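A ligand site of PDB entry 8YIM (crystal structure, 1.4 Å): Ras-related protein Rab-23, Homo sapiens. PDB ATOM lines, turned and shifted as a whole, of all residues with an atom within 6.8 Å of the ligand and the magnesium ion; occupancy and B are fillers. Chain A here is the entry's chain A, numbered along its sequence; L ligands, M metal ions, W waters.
Water W6 lies within hydrogen-bond range of O8 of the ligand (2.6 Å) and O of Lys 34 (2.8 Å). Water W4 bridges OD1 of Asp 59 and O of Thr 60. Water W7 lies within hydrogen-bond range of O8 of the ligand, N of Lys 34 and O of Asp 32. Water W3 lies within hydrogen-bond range of the side-chain amino group of Lys 35 (2.5 Å), an oxygen (O3) of the ligand (2.8 Å) and the backbone NH of Gln 63 (3.1 Å). Water W5 lies within hydrogen-bond range of O of Thr 30 (2.8 Å), O of Asp 32 (3.0 Å), OG of Ser 19 (3.4 Å) and O12 of the ligand (3.4 Å). Water W1 bridges NZ of Lys 117 (2.9 Å) and N6 of the ligand (3.4 Å).
NZ of Lys 17 sits at hydrogen-bond distance from O of Asn 12, 2.9 Å away. NZ of Lys 17 lies within hydrogen-bond range of O of Gly 11 (3.0 Å). OG1 of Thr 30 sits at hydrogen-bond distance from OD1 of Asp 32, at 2.8 Å. The backbone NH (N) of Val 147 sits close to the side-chain amide oxygen (OD1) of Asn 116 (3.5 Å). The side-chain carboxylate of Asp 119 lies within hydrogen-bond range of the side-chain hydroxyl of Ser 146, at 2.7 Å. O of Thr 145 sits at hydrogen-bond distance from N of Lys 117, 3.1 Å away. The backbone carbonyl oxygen of Val 15 lies within hydrogen-bond range of the side-chain amide nitrogen of Asn 116 (2.9 Å). The side-chain hydroxyl (OG) of Ser 146 lies within hydrogen-bond range of the backbone NH (N) of Glu 149, 3.0 Å away.
Two residues have an atom within 4 Å of the magnesium ion: Ser 18 and Thr 36. The nearest printed residue that does not touch the magnesium ion is Asp 59 (4.1 Å).
N of Thr 36 lies close to O1 of the ligand (3.2 Å). N of Ser 18 sits at hydrogen-bond distance from O7 of the ligand (3.5 Å). The side-chain hydroxyl (OH) of Tyr 33 lies within hydrogen-bond range of an oxygen (O3) of the ligand, 2.5 Å away. The backbone NH of Ser 19 sits at hydrogen-bond distance from an oxygen (O7) of the ligand (2.8 Å). The side-chain hydroxyl of Ser 19 is in hydrogen-bond range of an oxygen (O7) of the ligand (2.7 Å). N of Lys 17 is in hydrogen-bond range of O4 of the ligand (2.9 Å). The side-chain amino group (NZ) of Lys 17 is in salt-bridge range of an oxygen (O4) of the ligand (2.7 Å). O of Lys 31 sits at hydrogen-bond distance from O11 of the ligand (2.7 Å). The backbone carbonyl oxygen (O) of Thr 30 is in hydrogen-bond range of an oxygen (O12) of the ligand (2.8 Å). N of Val 147 sits at hydrogen-bond distance from O13 of the ligand (2.8 Å). N of Gly 62 sits at hydrogen-bond distance from O2 of the ligand, at 2.8 Å. A nitrogen (N4) of the ligand lies within hydrogen-bond range of the side-chain carboxylate of Asp 119. An oxygen (O10) of the ligand sits at hydrogen-bond distance from the side-chain amino group (NZ) of Lys 117 (3.1 Å). A nitrogen (N3) of the ligand lies within hydrogen-bond range of the side-chain amide nitrogen (ND2) of Asn 116. An oxygen (O4) of the ligand is in hydrogen-bond range of the backbone NH of Gly 16 (3.1 Å). An oxygen (O4) of the ligand sits at hydrogen-bond distance from the backbone NH (N) of Val 15, 3.4 Å away. N of Lys 148 sits at hydrogen-bond distance from O13 of the ligand, at 3.5 Å.
The side-chain hydroxyl (OG1) of Thr 36 is bound to the magnesium ion, at 2.0 Å. O1 of the ligand binds the magnesium ion, 2.1 Å away. OG of Ser 18 is bound to the magnesium ion (2.1 Å). The magnesium ion is bound by water W4. Water W6 is bound to the magnesium ion (2.1 Å). O5 of the ligand binds the magnesium ion (2.1 Å). The magnesium ion has six donor atoms within binding distance.
The backbone NH (N) of Ala 14 sits close to a nitrogen (N1) of the ligand, 3.0 Å away. Merely in contact with the ligand: Phe 29, Gly 13, Lys 35, Ser 146, Ala 61, Leu 120, Asp 32, Asn 12 and Lys 34. Hydrophobic or aromatic side chains within 4 Å of the ligand: Val 15, Phe 29, Tyr 33, Ala 61, Leu 120 and Val 147. 25 residues have an atom within 4 Å of the ligand: Asn 12, Gly 13, Ala 14, Val 15, Gly 16, Lys 17, Ser 18, Ser 19, Phe 29, Thr 30, Lys 31, Asp 32, Tyr 33, Lys 34, Lys 35, Thr 36, Ala 61, Gly 62, Asn 116, Lys 117, Asp 119, Leu 120, Ser 146, Val 147 and Lys 148. The nearest printed residue that does not touch the ligand is Thr 60 (4.4 Å).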
ATOM      1  N   GLY A  11     -12.101  -1.194 -14.424  1.00  0.00           N
ATOM      2  CA  GLY A  11     -12.096  -0.137 -15.418  1.00  0.00           C
ATOM      3  C   GLY A  11     -12.542   1.159 -14.786  1.00  0.00           C
ATOM      4  O   GLY A  11     -13.090   1.197 -13.693  1.00  0.00           O
ATOM      5  N   ASN A  12     -12.308   2.240 -15.517  1.00  0.00           N
ATOM      6  CA  ASN A  12     -12.588   3.574 -14.992  1.00  0.00           C
ATOM      7  C   ASN A  12     -14.069   3.740 -14.659  1.00  0.00           C
ATOM      8  O   ASN A  12     -14.936   2.985 -15.121  1.00  0.00           O
ATOM      9  CB  ASN A  12     -12.165   4.637 -15.995  1.00  0.00           C
ATOM     10  CG  ASN A  12     -10.695   4.981 -15.896  1.00  0.00           C
ATOM     11  OD1 ASN A  12      -9.922   4.220 -15.321  1.00  0.00           O
ATOM     12  ND2 ASN A  12     -10.313   6.127 -16.449  1.00  0.00           N
ATOM     13  N   GLY A  13     -14.352   4.748 -13.846  1.00  0.00           N
ATOM     14  CA  GLY A  13     -15.737   5.041 -13.501  1.00  0.00           C
ATOM     15  C   GLY A  13     -16.577   5.278 -14.746  1.00  0.00           C
ATOM     16  O   GLY A  13     -16.125   5.877 -15.717  1.00  0.00           O
ATOM     17  N   ALA A  14     -17.804   4.752 -14.713  1.00  0.00           N
ATOM     18  CA  ALA A  14     -18.836   4.972 -15.710  1.00  0.00           C
ATOM     19  C   ALA A  14     -18.615   4.226 -17.028  1.00  0.00           C
ATOM     20  O   ALA A  14     -19.355   4.470 -17.985  1.00  0.00           O
ATOM     21  CB  ALA A  14     -19.131   6.455 -15.968  1.00  0.00           C
ATOM     22  N   VAL A  15     -17.651   3.314 -17.108  1.00  0.00           N
ATOM     23  CA  VAL A  15     -17.460   2.562 -18.350  1.00  0.00           C
ATOM     24  C   VAL A  15     -18.568   1.537 -18.568  1.00  0.00           C
ATOM     25  O   VAL A  15     -18.743   1.057 -19.699  1.00  0.00           O
ATOM     26  CB  VAL A  15     -16.071   1.908 -18.477  1.00  0.00           C
ATOM     27  CG1 VAL A  15     -14.977   2.956 -18.422  1.00  0.00           C
ATOM     28  CG2 VAL A  15     -15.873   0.854 -17.389  1.00  0.00           C
ATOM     29  N   GLY A  16     -19.295   1.171 -17.530  1.00  0.00           N
ATOM     30  CA  GLY A  16     -20.379   0.219 -17.622  1.00  0.00           C
ATOM     31  C   GLY A  16     -20.174  -1.095 -16.905  1.00  0.00           C
ATOM     32  O   GLY A  16     -20.817  -2.089 -17.267  1.00  0.00           O
ATOM     33  N   LYS A  17     -19.291  -1.144 -15.889  1.00  0.00           N
ATOM     34  CA  LYS A  17     -19.019  -2.389 -15.192  1.00  0.00           C
ATOM     35  C   LYS A  17     -20.265  -2.943 -14.517  1.00  0.00           C
ATOM     36  O   LYS A  17     -20.628  -4.106 -14.712  1.00  0.00           O
ATOM     37  CB  LYS A  17     -17.909  -2.164 -14.157  1.00  0.00           C
ATOM     38  CG  LYS A  17     -16.619  -1.627 -14.745  1.00  0.00           C
ATOM     39  CD  LYS A  17     -15.532  -1.438 -13.690  1.00  0.00           C
ATOM     40  CE  LYS A  17     -15.874  -0.356 -12.667  1.00  0.00           C
ATOM     41  NZ  LYS A  17     -16.056   0.990 -13.297  1.00  0.00           N
ATOM     42  N   SER A  18     -20.953  -2.102 -13.729  1.00  0.00           N
ATOM     43  CA  SER A  18     -22.151  -2.549 -13.046  1.00  0.00           C
ATOM     44  C   SER A  18     -23.238  -2.927 -14.049  1.00  0.00           C
ATOM     45  O   SER A  18     -23.947  -3.920 -13.862  1.00  0.00           O
ATOM     46  CB  SER A  18     -22.667  -1.465 -12.116  1.00  0.00           C
ATOM     47  OG  SER A  18     -21.727  -1.163 -11.111  1.00  0.00           O
ATOM     48  N   SER A  19     -23.369  -2.138 -15.111  1.00  0.00           N
ATOM     49  CA  SER A  19     -24.370  -2.444 -16.135  1.00  0.00           C
ATOM     50  C   SER A  19     -24.104  -3.805 -16.757  1.00  0.00           C
ATOM     51  O   SER A  19     -25.027  -4.594 -16.967  1.00  0.00           O
ATOM     52  CB  SER A  19     -24.382  -1.350 -17.198  1.00  0.00           C
ATOM     53  OG  SER A  19     -24.777  -0.099 -16.666  1.00  0.00           O
ATOM     54  N   MET A  20     -22.831  -4.099 -17.082  1.00  0.00           N
ATOM     55  CA  MET A  20     -22.477  -5.397 -17.653  1.00  0.00           C
ATOM     56  C   MET A  20     -22.887  -6.520 -16.708  1.00  0.00           C
ATOM     57  O   MET A  20     -23.558  -7.478 -17.118  1.00  0.00           O
ATOM     58  CB  MET A  20     -20.977  -5.468 -17.914  1.00  0.00           C
ATOM     59  CG  MET A  20     -20.486  -4.663 -19.108  1.00  0.00           C
ATOM     60  SD  MET A  20     -18.705  -4.753 -19.389  1.00  0.00           S
ATOM     61  CE  MET A  20     -18.545  -6.430 -20.005  1.00  0.00           C
ATOM     62  N   PHE A  29     -31.214  -3.378 -17.875  1.00  0.00           N
ATOM     63  CA  PHE A  29     -30.328  -2.251 -18.130  1.00  0.00           C
ATOM     64  C   PHE A  29     -31.117  -0.966 -17.898  1.00  0.00           C
ATOM     65  O   PHE A  29     -32.270  -0.869 -18.317  1.00  0.00           O
ATOM     66  CB  PHE A  29     -29.802  -2.270 -19.561  1.00  0.00           C
ATOM     67  CG  PHE A  29     -29.066  -1.014 -19.956  1.00  0.00           C
ATOM     68  CD1 PHE A  29     -27.751  -0.818 -19.569  1.00  0.00           C
ATOM     69  CD2 PHE A  29     -29.690  -0.037 -20.724  1.00  0.00           C
ATOM     70  CE1 PHE A  29     -27.074   0.331 -19.927  1.00  0.00           C
ATOM     71  CE2 PHE A  29     -29.015   1.121 -21.079  1.00  0.00           C
ATOM     72  CZ  PHE A  29     -27.706   1.298 -20.678  1.00  0.00           C
ATOM     73  N   THR A  30     -30.501   0.000 -17.230  1.00  0.00           N
ATOM     74  CA  THR A  30     -31.095   1.330 -17.082  1.00  0.00           C
ATOM     75  C   THR A  30     -30.095   2.403 -17.488  1.00  0.00           C
ATOM     76  O   THR A  30     -28.875   2.201 -17.434  1.00  0.00           O
ATOM     77  CB  THR A  30     -31.625   1.609 -15.662  1.00  0.00           C
ATOM     78  OG1 THR A  30     -30.535   1.785 -14.754  1.00  0.00           O
ATOM     79  CG2 THR A  30     -32.519   0.463 -15.165  1.00  0.00           C
ATOM     80  N   LYS A  31     -30.625   3.552 -17.889  1.00  0.00           N
ATOM     81  CA  LYS A  31     -29.821   4.639 -18.425  1.00  0.00           C
ATOM     82  C   LYS A  31     -29.235   5.543 -17.346  1.00  0.00           C
ATOM     83  O   LYS A  31     -28.248   6.241 -17.613  1.00  0.00           O
ATOM     84  CB  LYS A  31     -30.674   5.501 -19.375  1.00  0.00           C
ATOM     85  CG  LYS A  31     -31.112   4.774 -20.632  1.00  0.00           C
ATOM     86  CD  LYS A  31     -31.993   5.671 -21.500  1.00  0.00           C
ATOM     87  CE  LYS A  31     -31.258   6.929 -21.926  1.00  0.00           C
ATOM     88  NZ  LYS A  31     -32.101   7.793 -22.800  1.00  0.00           N
ATOM     89  N   ASP A  32     -29.812   5.567 -16.158  1.00  0.00           N
ATOM     90  CA  ASP A  32     -29.337   6.463 -15.117  1.00  0.00           C
ATOM     91  C   ASP A  32     -28.066   5.904 -14.498  1.00  0.00           C
ATOM     92  O   ASP A  32     -27.929   4.690 -14.299  1.00  0.00           O
ATOM     93  CB  ASP A  32     -30.393   6.626 -14.027  1.00  0.00           C
ATOM     94  CG  ASP A  32     -30.752   5.322 -13.357  1.00  0.00           C
ATOM     95  OD1 ASP A  32     -31.233   4.396 -14.052  1.00  0.00           O
ATOM     96  OD2 ASP A  32     -30.521   5.206 -12.132  1.00  0.00           O
ATOM     97  N   TYR A  33     -27.123   6.790 -14.173  1.00  0.00           N
ATOM     98  CA  TYR A  33     -25.838   6.408 -13.623  1.00  0.00           C
ATOM     99  C   TYR A  33     -25.891   6.506 -12.110  1.00  0.00           C
ATOM    100  O   TYR A  33     -26.060   7.608 -11.560  1.00  0.00           O
ATOM    101  CB  TYR A  33     -24.728   7.307 -14.186  1.00  0.00           C
ATOM    102  CG  TYR A  33     -23.351   7.113 -13.587  1.00  0.00           C
ATOM    103  CD1 TYR A  33     -22.960   5.892 -13.042  1.00  0.00           C
ATOM    104  CD2 TYR A  33     -22.429   8.154 -13.576  1.00  0.00           C
ATOM    105  CE1 TYR A  33     -21.690   5.722 -12.500  1.00  0.00           C
ATOM    106  CE2 TYR A  33     -21.171   7.994 -13.039  1.00  0.00           C
ATOM    107  CZ  TYR A  33     -20.803   6.783 -12.499  1.00  0.00           C
ATOM    108  OH  TYR A  33     -19.539   6.642 -11.977  1.00  0.00           O
ATOM    109  N   LYS A  34     -25.734   5.368 -11.436  1.00  0.00           N
ATOM    110  CA  LYS A  34     -25.573   5.328  -9.987  1.00  0.00           C
ATOM    111  C   LYS A  34     -24.212   4.698  -9.699  1.00  0.00           C
ATOM    112  O   LYS A  34     -24.007   3.512  -9.961  1.00  0.00           O
ATOM    113  CB  LYS A  34     -26.703   4.522  -9.340  1.00  0.00           C
ATOM    114  CG  LYS A  34     -28.076   5.158  -9.494  1.00  0.00           C
ATOM    115  N   LYS A  35     -23.285   5.507  -9.177  1.00  0.00           N
ATOM    116  CA  LYS A  35     -21.974   5.009  -8.808  1.00  0.00           C
ATOM    117  C   LYS A  35     -22.098   3.883  -7.790  1.00  0.00           C
ATOM    118  O   LYS A  35     -22.917   3.949  -6.869  1.00  0.00           O
ATOM    119  CB  LYS A  35     -21.137   6.141  -8.230  1.00  0.00           C
ATOM    120  CG  LYS A  35     -19.719   5.760  -7.821  1.00  0.00           C
ATOM    121  CD  LYS A  35     -19.021   6.919  -7.144  1.00  0.00           C
ATOM    122  CE  LYS A  35     -17.689   6.506  -6.524  1.00  0.00           C
ATOM    123  NZ  LYS A  35     -16.656   6.205  -7.539  1.00  0.00           N
ATOM    124  N   THR A  36     -21.292   2.848  -7.973  1.00  0.00           N
ATOM    125  CA  THR A  36     -21.403   1.669  -7.108  1.00  0.00           C
ATOM    126  C   THR A  36     -20.919   1.985  -5.701  1.00  0.00           C
ATOM    127  O   THR A  36     -19.896   2.643  -5.500  1.00  0.00           O
ATOM    128  CB  THR A  36     -20.601   0.525  -7.706  1.00  0.00           C
ATOM    129  OG1 THR A  36     -21.164   0.191  -8.984  1.00  0.00           O
ATOM    130  CG2 THR A  36     -20.651  -0.703  -6.802  1.00  0.00           C
ATOM    131  N   ILE A  37     -21.684   1.512  -4.716  1.00  0.00           N
ATOM    132  CA  ILE A  37     -21.378   1.707  -3.301  1.00  0.00           C
ATOM    133  C   ILE A  37     -20.772   0.433  -2.753  1.00  0.00           C
ATOM    134  O   ILE A  37     -21.366  -0.655  -2.876  1.00  0.00           O
ATOM    135  CB  ILE A  37     -22.653   2.089  -2.516  1.00  0.00           C
ATOM    136  CG1 ILE A  37     -23.245   3.389  -3.066  1.00  0.00           C
ATOM    137  CG2 ILE A  37     -22.342   2.208  -1.025  1.00  0.00           C
ATOM    138  CD1 ILE A  37     -22.290   4.564  -3.012  1.00  0.00           C
ATOM    139  N   ASP A  59     -18.411  -6.523  -7.948  1.00  0.00           N
ATOM    140  CA  ASP A  59     -18.594  -5.222  -8.575  1.00  0.00           C
ATOM    141  C   ASP A  59     -18.213  -4.121  -7.592  1.00  0.00           C
ATOM    142  O   ASP A  59     -18.679  -4.135  -6.440  1.00  0.00           O
ATOM    143  CB  ASP A  59     -20.057  -5.062  -8.985  1.00  0.00           C
ATOM    144  CG  ASP A  59     -20.312  -3.842  -9.846  1.00  0.00           C
ATOM    145  OD1 ASP A  59     -19.431  -3.441 -10.631  1.00  0.00           O
ATOM    146  OD2 ASP A  59     -21.418  -3.270  -9.745  1.00  0.00           O
ATOM    147  N   THR A  60     -17.390  -3.175  -8.025  1.00  0.00           N
ATOM    148  CA  THR A  60     -17.038  -2.035  -7.198  1.00  0.00           C
ATOM    149  C   THR A  60     -16.745  -0.842  -8.104  1.00  0.00           C
ATOM    150  O   THR A  60     -16.507  -1.004  -9.300  1.00  0.00           O
ATOM    151  CB  THR A  60     -15.859  -2.365  -6.259  1.00  0.00           C
ATOM    152  OG1 THR A  60     -15.855  -1.469  -5.146  1.00  0.00           O
ATOM    153  CG2 THR A  60     -14.525  -2.267  -6.990  1.00  0.00           C
ATOM    154  N   ALA A  61     -16.812   0.358  -7.522  1.00  0.00           N
ATOM    155  CA  ALA A  61     -16.616   1.569  -8.315  1.00  0.00           C
ATOM    156  C   ALA A  61     -15.176   1.687  -8.785  1.00  0.00           C
ATOM    157  O   ALA A  61     -14.227   1.292  -8.093  1.00  0.00           O
ATOM    158  CB  ALA A  61     -16.991   2.808  -7.516  1.00  0.00           C
ATOM    159  N   GLY A  62     -15.005   2.267  -9.981  1.00  0.00           N
ATOM    160  CA  GLY A  62     -13.687   2.389 -10.571  1.00  0.00           C
ATOM    161  C   GLY A  62     -12.885   3.596 -10.133  1.00  0.00           C
ATOM    162  O   GLY A  62     -11.652   3.574 -10.232  1.00  0.00           O
ATOM    163  N   GLN A  63     -13.543   4.644  -9.652  1.00  0.00           N
ATOM    164  CA  GLN A  63     -12.824   5.854  -9.260  1.00  0.00           C
ATOM    165  C   GLN A  63     -12.032   5.646  -7.978  1.00  0.00           C
ATOM    166  O   GLN A  63     -12.456   4.920  -7.083  1.00  0.00           O
ATOM    167  CB  GLN A  63     -13.794   7.031  -9.102  1.00  0.00           C
ATOM    168  N   VAL A  83     -12.389  -3.373 -18.734  1.00  0.00           N
ATOM    169  CA  VAL A  83     -13.418  -2.651 -19.478  1.00  0.00           C
ATOM    170  C   VAL A  83     -12.966  -1.222 -19.723  1.00  0.00           C
ATOM    171  O   VAL A  83     -12.516  -0.536 -18.800  1.00  0.00           O
ATOM    172  CB  VAL A  83     -14.773  -2.652 -18.748  1.00  0.00           C
ATOM    173  CG1 VAL A  83     -15.852  -2.027 -19.626  1.00  0.00           C
ATOM    174  CG2 VAL A  83     -15.160  -4.056 -18.324  1.00  0.00           C
ATOM    175  N   ASN A 116     -16.845  -1.386 -24.124  1.00  0.00           N
ATOM    176  CA  ASN A 116     -18.276  -1.303 -23.907  1.00  0.00           C
ATOM    177  C   ASN A 116     -18.861  -0.035 -24.557  1.00  0.00           C
ATOM    178  O   ASN A 116     -18.127   0.853 -25.029  1.00  0.00           O
ATOM    179  CB  ASN A 116     -18.586  -1.344 -22.410  1.00  0.00           C
ATOM    180  CG  ASN A 116     -20.072  -1.483 -22.118  1.00  0.00           C
ATOM    181  OD1 ASN A 116     -20.783  -2.246 -22.791  1.00  0.00           O
ATOM    182  ND2 ASN A 116     -20.563  -0.756 -21.122  1.00  0.00           N
ATOM    183  N   LYS A 117     -20.185   0.037 -24.593  1.00  0.00           N
ATOM    184  CA  LYS A 117     -20.922   1.157 -25.184  1.00  0.00           C
ATOM    185  C   LYS A 117     -20.708   1.259 -26.691  1.00  0.00           C
ATOM    186  O   LYS A 117     -20.724   2.357 -27.253  1.00  0.00           O
ATOM    187  CB  LYS A 117     -20.633   2.503 -24.504  1.00  0.00           C
ATOM    188  CG  LYS A 117     -20.634   2.452 -22.982  1.00  0.00           C
ATOM    189  CD  LYS A 117     -20.775   3.853 -22.386  1.00  0.00           C
ATOM    190  CE  LYS A 117     -20.656   3.818 -20.867  1.00  0.00           C
ATOM    191  NZ  LYS A 117     -20.769   5.182 -20.278  1.00  0.00           N
ATOM    192  N   ILE A 118     -20.540   0.121 -27.365  1.00  0.00           N
ATOM    193  CA  ILE A 118     -20.296   0.129 -28.794  1.00  0.00           C
ATOM    194  C   ILE A 118     -21.492   0.676 -29.576  1.00  0.00           C
ATOM    195  O   ILE A 118     -21.346   1.041 -30.751  1.00  0.00           O
ATOM    196  CB  ILE A 118     -19.848  -1.272 -29.286  1.00  0.00           C
ATOM    197  CG1 ILE A 118     -19.053  -1.170 -30.580  1.00  0.00           C
ATOM    198  CG2 ILE A 118     -21.051  -2.192 -29.462  1.00  0.00           C
ATOM    199  CD1 ILE A 118     -17.668  -0.573 -30.390  1.00  0.00           C
ATOM    200  N   ASP A 119     -22.667   0.748 -28.950  1.00  0.00           N
ATOM    201  CA  ASP A 119     -23.828   1.362 -29.587  1.00  0.00           C
ATOM    202  C   ASP A 119     -23.657   2.863 -29.757  1.00  0.00           C
ATOM    203  O   ASP A 119     -24.397   3.476 -30.538  1.00  0.00           O
ATOM    204  CB  ASP A 119     -25.092   1.078 -28.776  1.00  0.00           C
ATOM    205  CG  ASP A 119     -24.975   1.533 -27.335  1.00  0.00           C
ATOM    206  OD1 ASP A 119     -24.265   0.864 -26.542  1.00  0.00           O
ATOM    207  OD2 ASP A 119     -25.570   2.573 -26.982  1.00  0.00           O
ATOM    208  N   LEU A 120     -22.721   3.480 -29.044  1.00  0.00           N
ATOM    209  CA  LEU A 120     -22.446   4.916 -29.141  1.00  0.00           C
ATOM    210  C   LEU A 120     -21.317   5.220 -30.117  1.00  0.00           C
ATOM    211  O   LEU A 120     -20.537   6.152 -29.901  1.00  0.00           O
ATOM    212  CB  LEU A 120     -22.138   5.482 -27.756  1.00  0.00           C
ATOM    213  CG  LEU A 120     -23.210   5.292 -26.682  1.00  0.00           C
ATOM    214  CD1 LEU A 120     -22.764   5.933 -25.376  1.00  0.00           C
ATOM    215  CD2 LEU A 120     -24.544   5.854 -27.132  1.00  0.00           C
ATOM    216  N   THR A 145     -18.785  -4.745 -26.704  1.00  0.00           N
ATOM    217  CA  THR A 145     -20.093  -5.010 -26.110  1.00  0.00           C
ATOM    218  C   THR A 145     -20.970  -3.779 -26.132  1.00  0.00           C
ATOM    219  O   THR A 145     -20.489  -2.637 -26.140  1.00  0.00           O
ATOM    220  CB  THR A 145     -19.978  -5.499 -24.649  1.00  0.00           C
ATOM    221  OG1 THR A 145     -19.343  -4.484 -23.854  1.00  0.00           O
ATOM    222  CG2 THR A 145     -19.183  -6.776 -24.563  1.00  0.00           C
ATOM    223  N   SER A 146     -22.279  -4.022 -26.126  1.00  0.00           N
ATOM    224  CA  SER A 146     -23.266  -3.010 -25.753  1.00  0.00           C
ATOM    225  C   SER A 146     -24.171  -3.642 -24.704  1.00  0.00           C
ATOM    226  O   SER A 146     -24.922  -4.564 -25.005  1.00  0.00           O
ATOM    227  CB  SER A 146     -24.102  -2.549 -26.948  1.00  0.00           C
ATOM    228  OG  SER A 146     -25.146  -1.704 -26.499  1.00  0.00           O
ATOM    229  N   VAL A 147     -24.082  -3.147 -23.472  1.00  0.00           N
ATOM    230  CA  VAL A 147     -25.024  -3.605 -22.456  1.00  0.00           C
ATOM    231  C   VAL A 147     -26.445  -3.167 -22.819  1.00  0.00           C
ATOM    232  O   VAL A 147     -27.413  -3.906 -22.603  1.00  0.00           O
ATOM    233  CB  VAL A 147     -24.612  -3.095 -21.070  1.00  0.00           C
ATOM    234  CG1 VAL A 147     -25.558  -3.635 -20.023  1.00  0.00           C
ATOM    235  CG2 VAL A 147     -23.198  -3.499 -20.790  1.00  0.00           C
ATOM    236  N   LYS A 148     -26.569  -1.954 -23.368  1.00  0.00           N
ATOM    237  CA  LYS A 148     -27.883  -1.439 -23.751  1.00  0.00           C
ATOM    238  C   LYS A 148     -28.575  -2.374 -24.737  1.00  0.00           C
ATOM    239  O   LYS A 148     -29.760  -2.673 -24.590  1.00  0.00           O
ATOM    240  CB  LYS A 148     -27.718  -0.040 -24.354  1.00  0.00           C
ATOM    241  CG  LYS A 148     -29.012   0.571 -24.873  1.00  0.00           C
ATOM    242  CD  LYS A 148     -28.761   1.950 -25.437  1.00  0.00           C
ATOM    243  CE  LYS A 148     -30.059   2.581 -25.926  1.00  0.00           C
ATOM    244  NZ  LYS A 148     -29.839   3.956 -26.446  1.00  0.00           N
ATOM    245  N   GLU A 149     -27.841  -2.853 -25.747  1.00  0.00           N
ATOM    246  CA  GLU A 149     -28.404  -3.720 -26.769  1.00  0.00           C
ATOM    247  C   GLU A 149     -28.263  -5.196 -26.451  1.00  0.00           C
ATOM    248  O   GLU A 149     -28.703  -6.027 -27.240  1.00  0.00           O
ATOM    249  CB  GLU A 149     -27.739  -3.434 -28.117  1.00  0.00           C
ATOM    250  CG  GLU A 149     -27.957  -2.018 -28.616  1.00  0.00           C
ATOM    251  CD  GLU A 149     -29.373  -1.791 -29.079  1.00  0.00           C
ATOM    252  OE1 GLU A 149     -29.801  -2.483 -30.029  1.00  0.00           O
ATOM    253  OE2 GLU A 149     -30.055  -0.925 -28.498  1.00  0.00           O
HETATM  254  P1  LIG L   1     -18.707   3.078 -11.371  1.00  0.00           P
HETATM  255  O1  LIG L   1     -19.406   2.157 -10.448  1.00  0.00           O
HETATM  256  O2  LIG L   1     -17.298   2.665 -11.583  1.00  0.00           O
HETATM  257  O3  LIG L   1     -18.830   4.495 -10.932  1.00  0.00           O
HETATM  258  N1  LIG L   1     -19.363   2.993 -12.885  1.00  0.00           N
HETATM  259  P2  LIG L   1     -19.645   1.669 -13.816  1.00  0.00           P
HETATM  260  O4  LIG L   1     -18.417   1.263 -14.543  1.00  0.00           O
HETATM  261  O5  LIG L   1     -20.256   0.581 -13.003  1.00  0.00           O
HETATM  262  O6  LIG L   1     -20.764   2.155 -14.880  1.00  0.00           O
HETATM  263  P3  LIG L   1     -22.351   1.976 -14.879  1.00  0.00           P
HETATM  264  O7  LIG L   1     -22.690   0.561 -15.170  1.00  0.00           O
HETATM  265  O8  LIG L   1     -22.877   2.618 -13.655  1.00  0.00           O
HETATM  266  O9  LIG L   1     -22.781   2.786 -16.190  1.00  0.00           O
HETATM  267  C1  LIG L   1     -22.457   4.187 -16.306  1.00  0.00           C
HETATM  268  C2  LIG L   1     -23.379   4.800 -17.332  1.00  0.00           C
HETATM  269  O10 LIG L   1     -23.139   4.202 -18.623  1.00  0.00           O
HETATM  270  C3  LIG L   1     -24.881   4.642 -17.058  1.00  0.00           C
HETATM  271  O11 LIG L   1     -25.565   5.839 -17.415  1.00  0.00           O
HETATM  272  C4  LIG L   1     -25.279   3.477 -17.979  1.00  0.00           C
HETATM  273  O12 LIG L   1     -26.636   3.573 -18.392  1.00  0.00           O
HETATM  274  C5  LIG L   1     -24.352   3.729 -19.167  1.00  0.00           C
HETATM  275  N2  LIG L   1     -24.066   2.518 -19.946  1.00  0.00           N
HETATM  276  C6  LIG L   1     -23.502   1.351 -19.512  1.00  0.00           C
HETATM  277  N3  LIG L   1     -23.317   0.473 -20.469  1.00  0.00           N
HETATM  278  C7  LIG L   1     -23.790   1.098 -21.604  1.00  0.00           C
HETATM  279  C8  LIG L   1     -23.841   0.667 -22.965  1.00  0.00           C
HETATM  280  O13 LIG L   1     -23.462  -0.412 -23.414  1.00  0.00           O
HETATM  281  N4  LIG L   1     -24.380   1.635 -23.798  1.00  0.00           N
HETATM  282  C9  LIG L   1     -24.821   2.867 -23.400  1.00  0.00           C
HETATM  283  N5  LIG L   1     -25.313   3.670 -24.340  1.00  0.00           N
HETATM  284  N6  LIG L   1     -24.776   3.282 -22.133  1.00  0.00           N
HETATM  285  C10 LIG L   1     -24.258   2.364 -21.298  1.00  0.00           C
HETATM  286 MG    MG M   1     -20.579   0.534 -10.910  1.00  0.00          MG
HETATM  287  O   HOH W   1     -23.210   6.207 -21.475  1.00  0.00           O
HETATM  288  O   HOH W   2     -24.459   8.328 -17.879  1.00  0.00           O
HETATM  289  O   HOH W   3     -16.458   5.557  -9.912  1.00  0.00           O
HETATM  290  O   HOH W   4     -18.965  -0.794 -10.706  1.00  0.00           O
HETATM  291  O   HOH W   5     -26.931   2.124 -15.365  1.00  0.00           O
HETATM  292  O   HOH W   6     -22.310   1.701 -11.237  1.00  0.00           O
HETATM  293  O   HOH W   7     -25.481   2.913 -13.079  1.00  0.00           O
